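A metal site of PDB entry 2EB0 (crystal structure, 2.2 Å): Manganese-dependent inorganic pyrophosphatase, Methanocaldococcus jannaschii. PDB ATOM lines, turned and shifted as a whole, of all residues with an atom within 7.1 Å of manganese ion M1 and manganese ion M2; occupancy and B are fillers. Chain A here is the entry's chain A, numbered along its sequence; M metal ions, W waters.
Water W1 bridges the side-chain carboxylate of Asp 147 and the side-chain carboxylate of Asp 11.
Residues that only touch manganese ion M2: Ser 14 (3.8 Å) and Lys 204 (3.5 Å).
Of the 25 residues printed, 5 come within 4 Å of manganese ion M2.
The nearest printed residue that does not touch manganese ion M2 is Asp 147 (4.5 Å).
Residues that only touch manganese ion M1: Thr 109.
Along chain A the residues within 4 Å of manganese ion M1 span positions 13 to 147.
The nearest printed residue that does not touch manganese ion M1 is Ser 108 (4.2 Å).
The side-chain carboxylate of Asp 11 sits close to a ring nitrogen (NE2) of His 7 (3.1 Å).
N of Thr 109 sits close to OD2 of Asp 13 (3.4 Å).
The backbone NH (N) of Asp 66 lies close to the side-chain hydroxyl (OG1) of Thr 109 (3.4 Å).
The backbone carbonyl oxygen of His 88 sits at hydrogen-bond distance from the side-chain amino group of Lys 294.
ND1 of His 7 lies close to O of Asn 9.
The side-chain hydroxyl (OG) of Ser 14 lies close to the backbone NH (N) of His 7 (3.4 Å).
The side-chain carboxylate of Asp 13 sits at hydrogen-bond distance from the backbone NH of Ala 110, at 3.0 Å.
OG of Ser 14 lies within hydrogen-bond range of OD1 of Asp 11 (3.0 Å).
OD1 of Asp 13 is bound to manganese ion M1, 2.2 Å away.
Manganese ion M1 is bound by water W1, 2.3 Å away.
Manganese ion M1 is bound by OD2 of Asp 147 (2.3 Å).
OD2 of Asp 66 is bound to manganese ion M1, at 2.4 Å.
NE2 of His 88 is bound to manganese ion M1, 2.5 Å away.
Manganese ion M2 is bound by the side-chain carboxylate (OD1) of Asp 66 (2.3 Å), water W1 (2.3 Å) and a ring nitrogen (NE2) of His 7 (2.4 Å).
Manganese ion M2 has three donor atoms within binding distance.
Slightly farther from manganese ion M2 lies OD2 of Asp 11 (2.7 Å).
Slightly farther from manganese ion M2 lies the side-chain carboxylate (OD1) of Asp 11 (2.8 Å).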
ATOM      1  N   HIS A   7     -21.801   5.678 -14.171  1.00  0.00           N
ATOM      2  CA  HIS A   7     -20.683   5.752 -15.124  1.00  0.00           C
ATOM      3  C   HIS A   7     -20.042   7.144 -15.188  1.00  0.00           C
ATOM      4  O   HIS A   7     -20.570   8.110 -14.629  1.00  0.00           O
ATOM      5  CB  HIS A   7     -21.170   5.330 -16.528  1.00  0.00           C
ATOM      6  CG  HIS A   7     -22.350   6.102 -17.020  1.00  0.00           C
ATOM      7  ND1 HIS A   7     -22.275   7.440 -17.366  1.00  0.00           N
ATOM      8  CD2 HIS A   7     -23.640   5.739 -17.196  1.00  0.00           C
ATOM      9  CE1 HIS A   7     -23.476   7.864 -17.713  1.00  0.00           C
ATOM     10  NE2 HIS A   7     -24.321   6.852 -17.618  1.00  0.00           N
ATOM     11  N   LYS A   8     -18.898   7.230 -15.856  1.00  0.00           N
ATOM     12  CA  LYS A   8     -18.211   8.522 -16.014  1.00  0.00           C
ATOM     13  C   LYS A   8     -19.180   9.390 -16.797  1.00  0.00           C
ATOM     14  O   LYS A   8     -20.077   8.864 -17.475  1.00  0.00           O
ATOM     15  CB  LYS A   8     -16.916   8.378 -16.802  1.00  0.00           C
ATOM     16  CG  LYS A   8     -15.886   7.430 -16.217  1.00  0.00           C
ATOM     17  CD  LYS A   8     -14.534   7.692 -16.872  1.00  0.00           C
ATOM     18  CE  LYS A   8     -13.563   6.534 -16.683  1.00  0.00           C
ATOM     19  NZ  LYS A   8     -13.936   5.376 -17.559  1.00  0.00           N
ATOM     20  N   ASN A   9     -18.990  10.704 -16.735  1.00  0.00           N
ATOM     21  CA  ASN A   9     -19.898  11.638 -17.420  1.00  0.00           C
ATOM     22  C   ASN A   9     -21.307  11.155 -17.066  1.00  0.00           C
ATOM     23  O   ASN A   9     -22.121  10.817 -17.932  1.00  0.00           O
ATOM     24  CB  ASN A   9     -19.662  11.619 -18.932  1.00  0.00           C
ATOM     25  CG  ASN A   9     -18.246  12.042 -19.309  1.00  0.00           C
ATOM     26  OD1 ASN A   9     -17.653  12.918 -18.670  1.00  0.00           O
ATOM     27  ND2 ASN A   9     -17.684  11.424 -20.343  1.00  0.00           N
ATOM     28  N   PRO A  10     -21.603  11.101 -15.763  1.00  0.00           N
ATOM     29  CA  PRO A  10     -22.900  10.655 -15.287  1.00  0.00           C
ATOM     30  C   PRO A  10     -24.070  11.472 -15.786  1.00  0.00           C
ATOM     31  O   PRO A  10     -23.992  12.679 -15.973  1.00  0.00           O
ATOM     32  CB  PRO A  10     -22.751  10.720 -13.762  1.00  0.00           C
ATOM     33  CG  PRO A  10     -21.797  11.871 -13.559  1.00  0.00           C
ATOM     34  CD  PRO A  10     -20.775  11.625 -14.657  1.00  0.00           C
ATOM     35  N   ASP A  11     -25.166  10.772 -16.032  1.00  0.00           N
ATOM     36  CA  ASP A  11     -26.399  11.385 -16.478  1.00  0.00           C
ATOM     37  C   ASP A  11     -27.338  11.270 -15.269  1.00  0.00           C
ATOM     38  O   ASP A  11     -26.912  10.812 -14.200  1.00  0.00           O
ATOM     39  CB  ASP A  11     -26.955  10.596 -17.661  1.00  0.00           C
ATOM     40  CG  ASP A  11     -27.255   9.152 -17.325  1.00  0.00           C
ATOM     41  OD1 ASP A  11     -26.562   8.581 -16.445  1.00  0.00           O
ATOM     42  OD2 ASP A  11     -28.168   8.584 -17.945  1.00  0.00           O
ATOM     43  N   THR A  12     -28.581  11.661 -15.430  1.00  0.00           N
ATOM     44  CA  THR A  12     -29.514  11.616 -14.319  1.00  0.00           C
ATOM     45  C   THR A  12     -29.720  10.215 -13.752  1.00  0.00           C
ATOM     46  O   THR A  12     -29.759  10.042 -12.540  1.00  0.00           O
ATOM     47  CB  THR A  12     -30.853  12.261 -14.715  1.00  0.00           C
ATOM     48  OG1 THR A  12     -30.633  13.646 -14.974  1.00  0.00           O
ATOM     49  CG2 THR A  12     -31.869  12.127 -13.592  1.00  0.00           C
ATOM     50  N   ASP A  13     -29.843   9.200 -14.613  1.00  0.00           N
ATOM     51  CA  ASP A  13     -30.054   7.852 -14.132  1.00  0.00           C
ATOM     52  C   ASP A  13     -28.922   7.417 -13.196  1.00  0.00           C
ATOM     53  O   ASP A  13     -29.168   6.843 -12.139  1.00  0.00           O
ATOM     54  CB  ASP A  13     -30.158   6.858 -15.284  1.00  0.00           C
ATOM     55  CG  ASP A  13     -30.808   5.549 -14.866  1.00  0.00           C
ATOM     56  OD1 ASP A  13     -30.673   4.535 -15.581  1.00  0.00           O
ATOM     57  OD2 ASP A  13     -31.481   5.539 -13.816  1.00  0.00           O
ATOM     58  N   SER A  14     -27.685   7.693 -13.607  1.00  0.00           N
ATOM     59  CA  SER A  14     -26.512   7.320 -12.822  1.00  0.00           C
ATOM     60  C   SER A  14     -26.458   8.014 -11.455  1.00  0.00           C
ATOM     61  O   SER A  14     -26.059   7.402 -10.465  1.00  0.00           O
ATOM     62  CB  SER A  14     -25.233   7.647 -13.591  1.00  0.00           C
ATOM     63  OG  SER A  14     -25.032   6.736 -14.655  1.00  0.00           O
ATOM     64  N   SER A  17     -29.911   6.871  -9.410  1.00  0.00           N
ATOM     65  CA  SER A  17     -29.825   5.470  -9.007  1.00  0.00           C
ATOM     66  C   SER A  17     -28.791   5.285  -7.912  1.00  0.00           C
ATOM     67  O   SER A  17     -29.000   4.497  -7.004  1.00  0.00           O
ATOM     68  CB  SER A  17     -29.483   4.566 -10.190  1.00  0.00           C
ATOM     69  OG  SER A  17     -30.583   4.427 -11.064  1.00  0.00           O
ATOM     70  N   VAL A  65     -24.017   1.100 -10.770  1.00  0.00           N
ATOM     71  CA  VAL A  65     -25.352   1.231 -11.314  1.00  0.00           C
ATOM     72  C   VAL A  65     -25.255   1.854 -12.693  1.00  0.00           C
ATOM     73  O   VAL A  65     -24.350   2.635 -12.989  1.00  0.00           O
ATOM     74  CB  VAL A  65     -26.276   2.146 -10.452  1.00  0.00           C
ATOM     75  CG1 VAL A  65     -26.588   1.444  -9.134  1.00  0.00           C
ATOM     76  CG2 VAL A  65     -25.626   3.517 -10.213  1.00  0.00           C
ATOM     77  N   ASP A  66     -26.168   1.435 -13.560  1.00  0.00           N
ATOM     78  CA  ASP A  66     -26.260   2.000 -14.877  1.00  0.00           C
ATOM     79  C   ASP A  66     -25.131   1.754 -15.893  1.00  0.00           C
ATOM     80  O   ASP A  66     -24.979   2.516 -16.846  1.00  0.00           O
ATOM     81  CB  ASP A  66     -26.466   3.498 -14.719  1.00  0.00           C
ATOM     82  CG  ASP A  66     -27.016   4.141 -15.943  1.00  0.00           C
ATOM     83  OD1 ASP A  66     -26.882   5.360 -16.052  1.00  0.00           O
ATOM     84  OD2 ASP A  66     -27.579   3.416 -16.787  1.00  0.00           O
ATOM     85  N   HIS A  67     -24.327   0.715 -15.684  1.00  0.00           N
ATOM     86  CA  HIS A  67     -23.276   0.416 -16.647  1.00  0.00           C
ATOM     87  C   HIS A  67     -22.525  -0.865 -16.333  1.00  0.00           C
ATOM     88  O   HIS A  67     -22.504  -1.317 -15.184  1.00  0.00           O
ATOM     89  CB  HIS A  67     -22.281   1.587 -16.784  1.00  0.00           C
ATOM     90  CG  HIS A  67     -21.329   1.753 -15.639  1.00  0.00           C
ATOM     91  ND1 HIS A  67     -21.731   2.138 -14.378  1.00  0.00           N
ATOM     92  CD2 HIS A  67     -19.987   1.583 -15.562  1.00  0.00           C
ATOM     93  CE1 HIS A  67     -20.682   2.214 -13.580  1.00  0.00           C
ATOM     94  NE2 HIS A  67     -19.600   1.882 -14.280  1.00  0.00           N
ATOM     95  N   ASP A  87     -28.247  -2.701 -13.390  1.00  0.00           N
ATOM     96  CA  ASP A  87     -28.174  -1.994 -14.658  1.00  0.00           C
ATOM     97  C   ASP A  87     -29.253  -2.435 -15.637  1.00  0.00           C
ATOM     98  O   ASP A  87     -30.092  -3.287 -15.316  1.00  0.00           O
ATOM     99  CB  ASP A  87     -26.781  -2.302 -15.227  1.00  0.00           C
ATOM    100  CG  ASP A  87     -26.483  -1.561 -16.492  1.00  0.00           C
ATOM    101  OD1 ASP A  87     -25.685  -2.087 -17.292  1.00  0.00           O
ATOM    102  OD2 ASP A  87     -27.026  -0.451 -16.684  1.00  0.00           O
ATOM    103  N   HIS A  88     -29.245  -1.842 -16.830  1.00  0.00           N
ATOM    104  CA  HIS A  88     -30.215  -2.177 -17.860  1.00  0.00           C
ATOM    105  C   HIS A  88     -29.546  -2.285 -19.232  1.00  0.00           C
ATOM    106  O   HIS A  88     -30.217  -2.320 -20.257  1.00  0.00           O
ATOM    107  CB  HIS A  88     -31.358  -1.167 -17.887  1.00  0.00           C
ATOM    108  CG  HIS A  88     -30.938   0.217 -18.270  1.00  0.00           C
ATOM    109  ND1 HIS A  88     -31.415   0.850 -19.405  1.00  0.00           N
ATOM    110  CD2 HIS A  88     -30.102   1.094 -17.674  1.00  0.00           C
ATOM    111  CE1 HIS A  88     -30.881   2.049 -19.492  1.00  0.00           C
ATOM    112  NE2 HIS A  88     -30.075   2.225 -18.459  1.00  0.00           N
ATOM    113  N   HIS A  89     -28.209  -2.332 -19.235  1.00  0.00           N
ATOM    114  CA  HIS A  89     -27.455  -2.460 -20.469  1.00  0.00           C
ATOM    115  C   HIS A  89     -27.072  -3.928 -20.666  1.00  0.00           C
ATOM    116  O   HIS A  89     -27.352  -4.774 -19.822  1.00  0.00           O
ATOM    117  CB  HIS A  89     -26.174  -1.622 -20.403  1.00  0.00           C
ATOM    118  CG  HIS A  89     -26.403  -0.144 -20.339  1.00  0.00           C
ATOM    119  ND1 HIS A  89     -26.788   0.495 -19.184  1.00  0.00           N
ATOM    120  CD2 HIS A  89     -26.322   0.816 -21.301  1.00  0.00           C
ATOM    121  CE1 HIS A  89     -26.935   1.789 -19.439  1.00  0.00           C
ATOM    122  NE2 HIS A  89     -26.665   2.001 -20.709  1.00  0.00           N
ATOM    123  N   GLY A 107     -36.111   0.587 -19.786  1.00  0.00           N
ATOM    124  CA  GLY A 107     -35.672   1.941 -20.118  1.00  0.00           C
ATOM    125  C   GLY A 107     -34.618   2.620 -19.261  1.00  0.00           C
ATOM    126  O   GLY A 107     -33.875   3.463 -19.764  1.00  0.00           O
ATOM    127  N   SER A 108     -34.545   2.299 -17.976  1.00  0.00           N
ATOM    128  CA  SER A 108     -33.545   2.940 -17.136  1.00  0.00           C
ATOM    129  C   SER A 108     -33.205   2.088 -15.937  1.00  0.00           C
ATOM    130  O   SER A 108     -33.866   1.087 -15.663  1.00  0.00           O
ATOM    131  CB  SER A 108     -34.069   4.293 -16.633  1.00  0.00           C
ATOM    132  OG  SER A 108     -35.073   4.107 -15.649  1.00  0.00           O
ATOM    133  N   THR A 109     -32.159   2.496 -15.215  1.00  0.00           N
ATOM    134  CA  THR A 109     -31.768   1.764 -14.020  1.00  0.00           C
ATOM    135  C   THR A 109     -32.779   2.113 -12.925  1.00  0.00           C
ATOM    136  O   THR A 109     -33.088   1.271 -12.079  1.00  0.00           O
ATOM    137  CB  THR A 109     -30.324   2.154 -13.578  1.00  0.00           C
ATOM    138  OG1 THR A 109     -29.391   1.790 -14.595  1.00  0.00           O
ATOM    139  CG2 THR A 109     -29.939   1.423 -12.279  1.00  0.00           C
ATOM    140  N   ALA A 110     -33.312   3.330 -12.956  1.00  0.00           N
ATOM    141  CA  ALA A 110     -34.303   3.753 -11.974  1.00  0.00           C
ATOM    142  C   ALA A 110     -35.544   2.871 -12.058  1.00  0.00           C
ATOM    143  O   ALA A 110     -36.150   2.519 -11.041  1.00  0.00           O
ATOM    144  CB  ALA A 110     -34.682   5.230 -12.193  1.00  0.00           C
ATOM    145  N   ALA A 143     -35.209  10.191 -13.529  1.00  0.00           N
ATOM    146  CA  ALA A 143     -34.267   9.297 -14.193  1.00  0.00           C
ATOM    147  C   ALA A 143     -34.972   8.559 -15.330  1.00  0.00           C
ATOM    148  O   ALA A 143     -34.448   8.450 -16.435  1.00  0.00           O
ATOM    149  CB  ALA A 143     -33.711   8.305 -13.181  1.00  0.00           C
ATOM    150  N   ASP A 147     -33.911   9.159 -19.064  1.00  0.00           N
ATOM    151  CA  ASP A 147     -33.453   7.994 -19.821  1.00  0.00           C
ATOM    152  C   ASP A 147     -34.308   7.585 -21.014  1.00  0.00           C
ATOM    153  O   ASP A 147     -33.792   7.081 -22.016  1.00  0.00           O
ATOM    154  CB  ASP A 147     -33.301   6.806 -18.879  1.00  0.00           C
ATOM    155  CG  ASP A 147     -31.879   6.382 -18.691  1.00  0.00           C
ATOM    156  OD1 ASP A 147     -30.981   7.260 -18.816  1.00  0.00           O
ATOM    157  OD2 ASP A 147     -31.654   5.191 -18.408  1.00  0.00           O
ATOM    158  N   ASP A 202     -21.699  14.233 -22.200  1.00  0.00           N
ATOM    159  CA  ASP A 202     -22.242  12.880 -22.258  1.00  0.00           C
ATOM    160  C   ASP A 202     -21.534  11.991 -23.278  1.00  0.00           C
ATOM    161  O   ASP A 202     -22.125  11.583 -24.279  1.00  0.00           O
ATOM    162  CB  ASP A 202     -23.735  12.940 -22.581  1.00  0.00           C
ATOM    163  CG  ASP A 202     -24.338  11.576 -22.831  1.00  0.00           C
ATOM    164  OD1 ASP A 202     -24.114  10.659 -22.024  1.00  0.00           O
ATOM    165  OD2 ASP A 202     -25.043  11.422 -23.850  1.00  0.00           O
ATOM    166  N   LYS A 204     -19.414   8.413 -24.066  1.00  0.00           N
ATOM    167  CA  LYS A 204     -19.192   7.062 -23.556  1.00  0.00           C
ATOM    168  C   LYS A 204     -18.154   6.318 -24.394  1.00  0.00           C
ATOM    169  O   LYS A 204     -18.086   6.501 -25.605  1.00  0.00           O
ATOM    170  CB  LYS A 204     -20.505   6.272 -23.515  1.00  0.00           C
ATOM    171  CG  LYS A 204     -21.386   6.630 -22.331  1.00  0.00           C
ATOM    172  CD  LYS A 204     -22.626   5.754 -22.221  1.00  0.00           C
ATOM    173  CE  LYS A 204     -23.347   6.028 -20.904  1.00  0.00           C
ATOM    174  NZ  LYS A 204     -24.646   5.284 -20.756  1.00  0.00           N
ATOM    175  N   ARG A 293     -28.447   5.597 -27.925  1.00  0.00           N
ATOM    176  CA  ARG A 293     -27.104   5.155 -28.275  1.00  0.00           C
ATOM    177  C   ARG A 293     -26.975   3.656 -28.051  1.00  0.00           C
ATOM    178  O   ARG A 293     -26.621   2.909 -28.963  1.00  0.00           O
ATOM    179  CB  ARG A 293     -26.066   5.891 -27.416  1.00  0.00           C
ATOM    180  CG  ARG A 293     -24.654   5.324 -27.467  1.00  0.00           C
ATOM    181  CD  ARG A 293     -23.712   6.210 -26.679  1.00  0.00           C
ATOM    182  NE  ARG A 293     -24.320   6.620 -25.416  1.00  0.00           N
ATOM    183  CZ  ARG A 293     -24.029   7.752 -24.783  1.00  0.00           C
ATOM    184  NH1 ARG A 293     -23.134   8.594 -25.289  1.00  0.00           N
ATOM    185  NH2 ARG A 293     -24.639   8.049 -23.648  1.00  0.00           N
ATOM    186  N   LYS A 294     -27.305   3.219 -26.841  1.00  0.00           N
ATOM    187  CA  LYS A 294     -27.215   1.818 -26.475  1.00  0.00           C
ATOM    188  C   LYS A 294     -28.015   0.879 -27.369  1.00  0.00           C
ATOM    189  O   LYS A 294     -27.526  -0.176 -27.782  1.00  0.00           O
ATOM    190  CB  LYS A 294     -27.691   1.612 -25.031  1.00  0.00           C
ATOM    191  CG  LYS A 294     -29.162   1.931 -24.815  1.00  0.00           C
ATOM    192  CD  LYS A 294     -29.610   1.511 -23.445  1.00  0.00           C
ATOM    193  CE  LYS A 294     -29.509   0.005 -23.275  1.00  0.00           C
ATOM    194  NZ  LYS A 294     -30.004  -0.419 -21.948  1.00  0.00           N
HETATM  195 MN    MN M   1     -29.631   4.499 -17.530  1.00  0.00          MN
HETATM  196 MN    MN M   2     -26.595   6.355 -18.074  1.00  0.00          MN
HETATM  197  O   HOH W   1     -28.580   5.791 -19.055  1.00  0.00           O
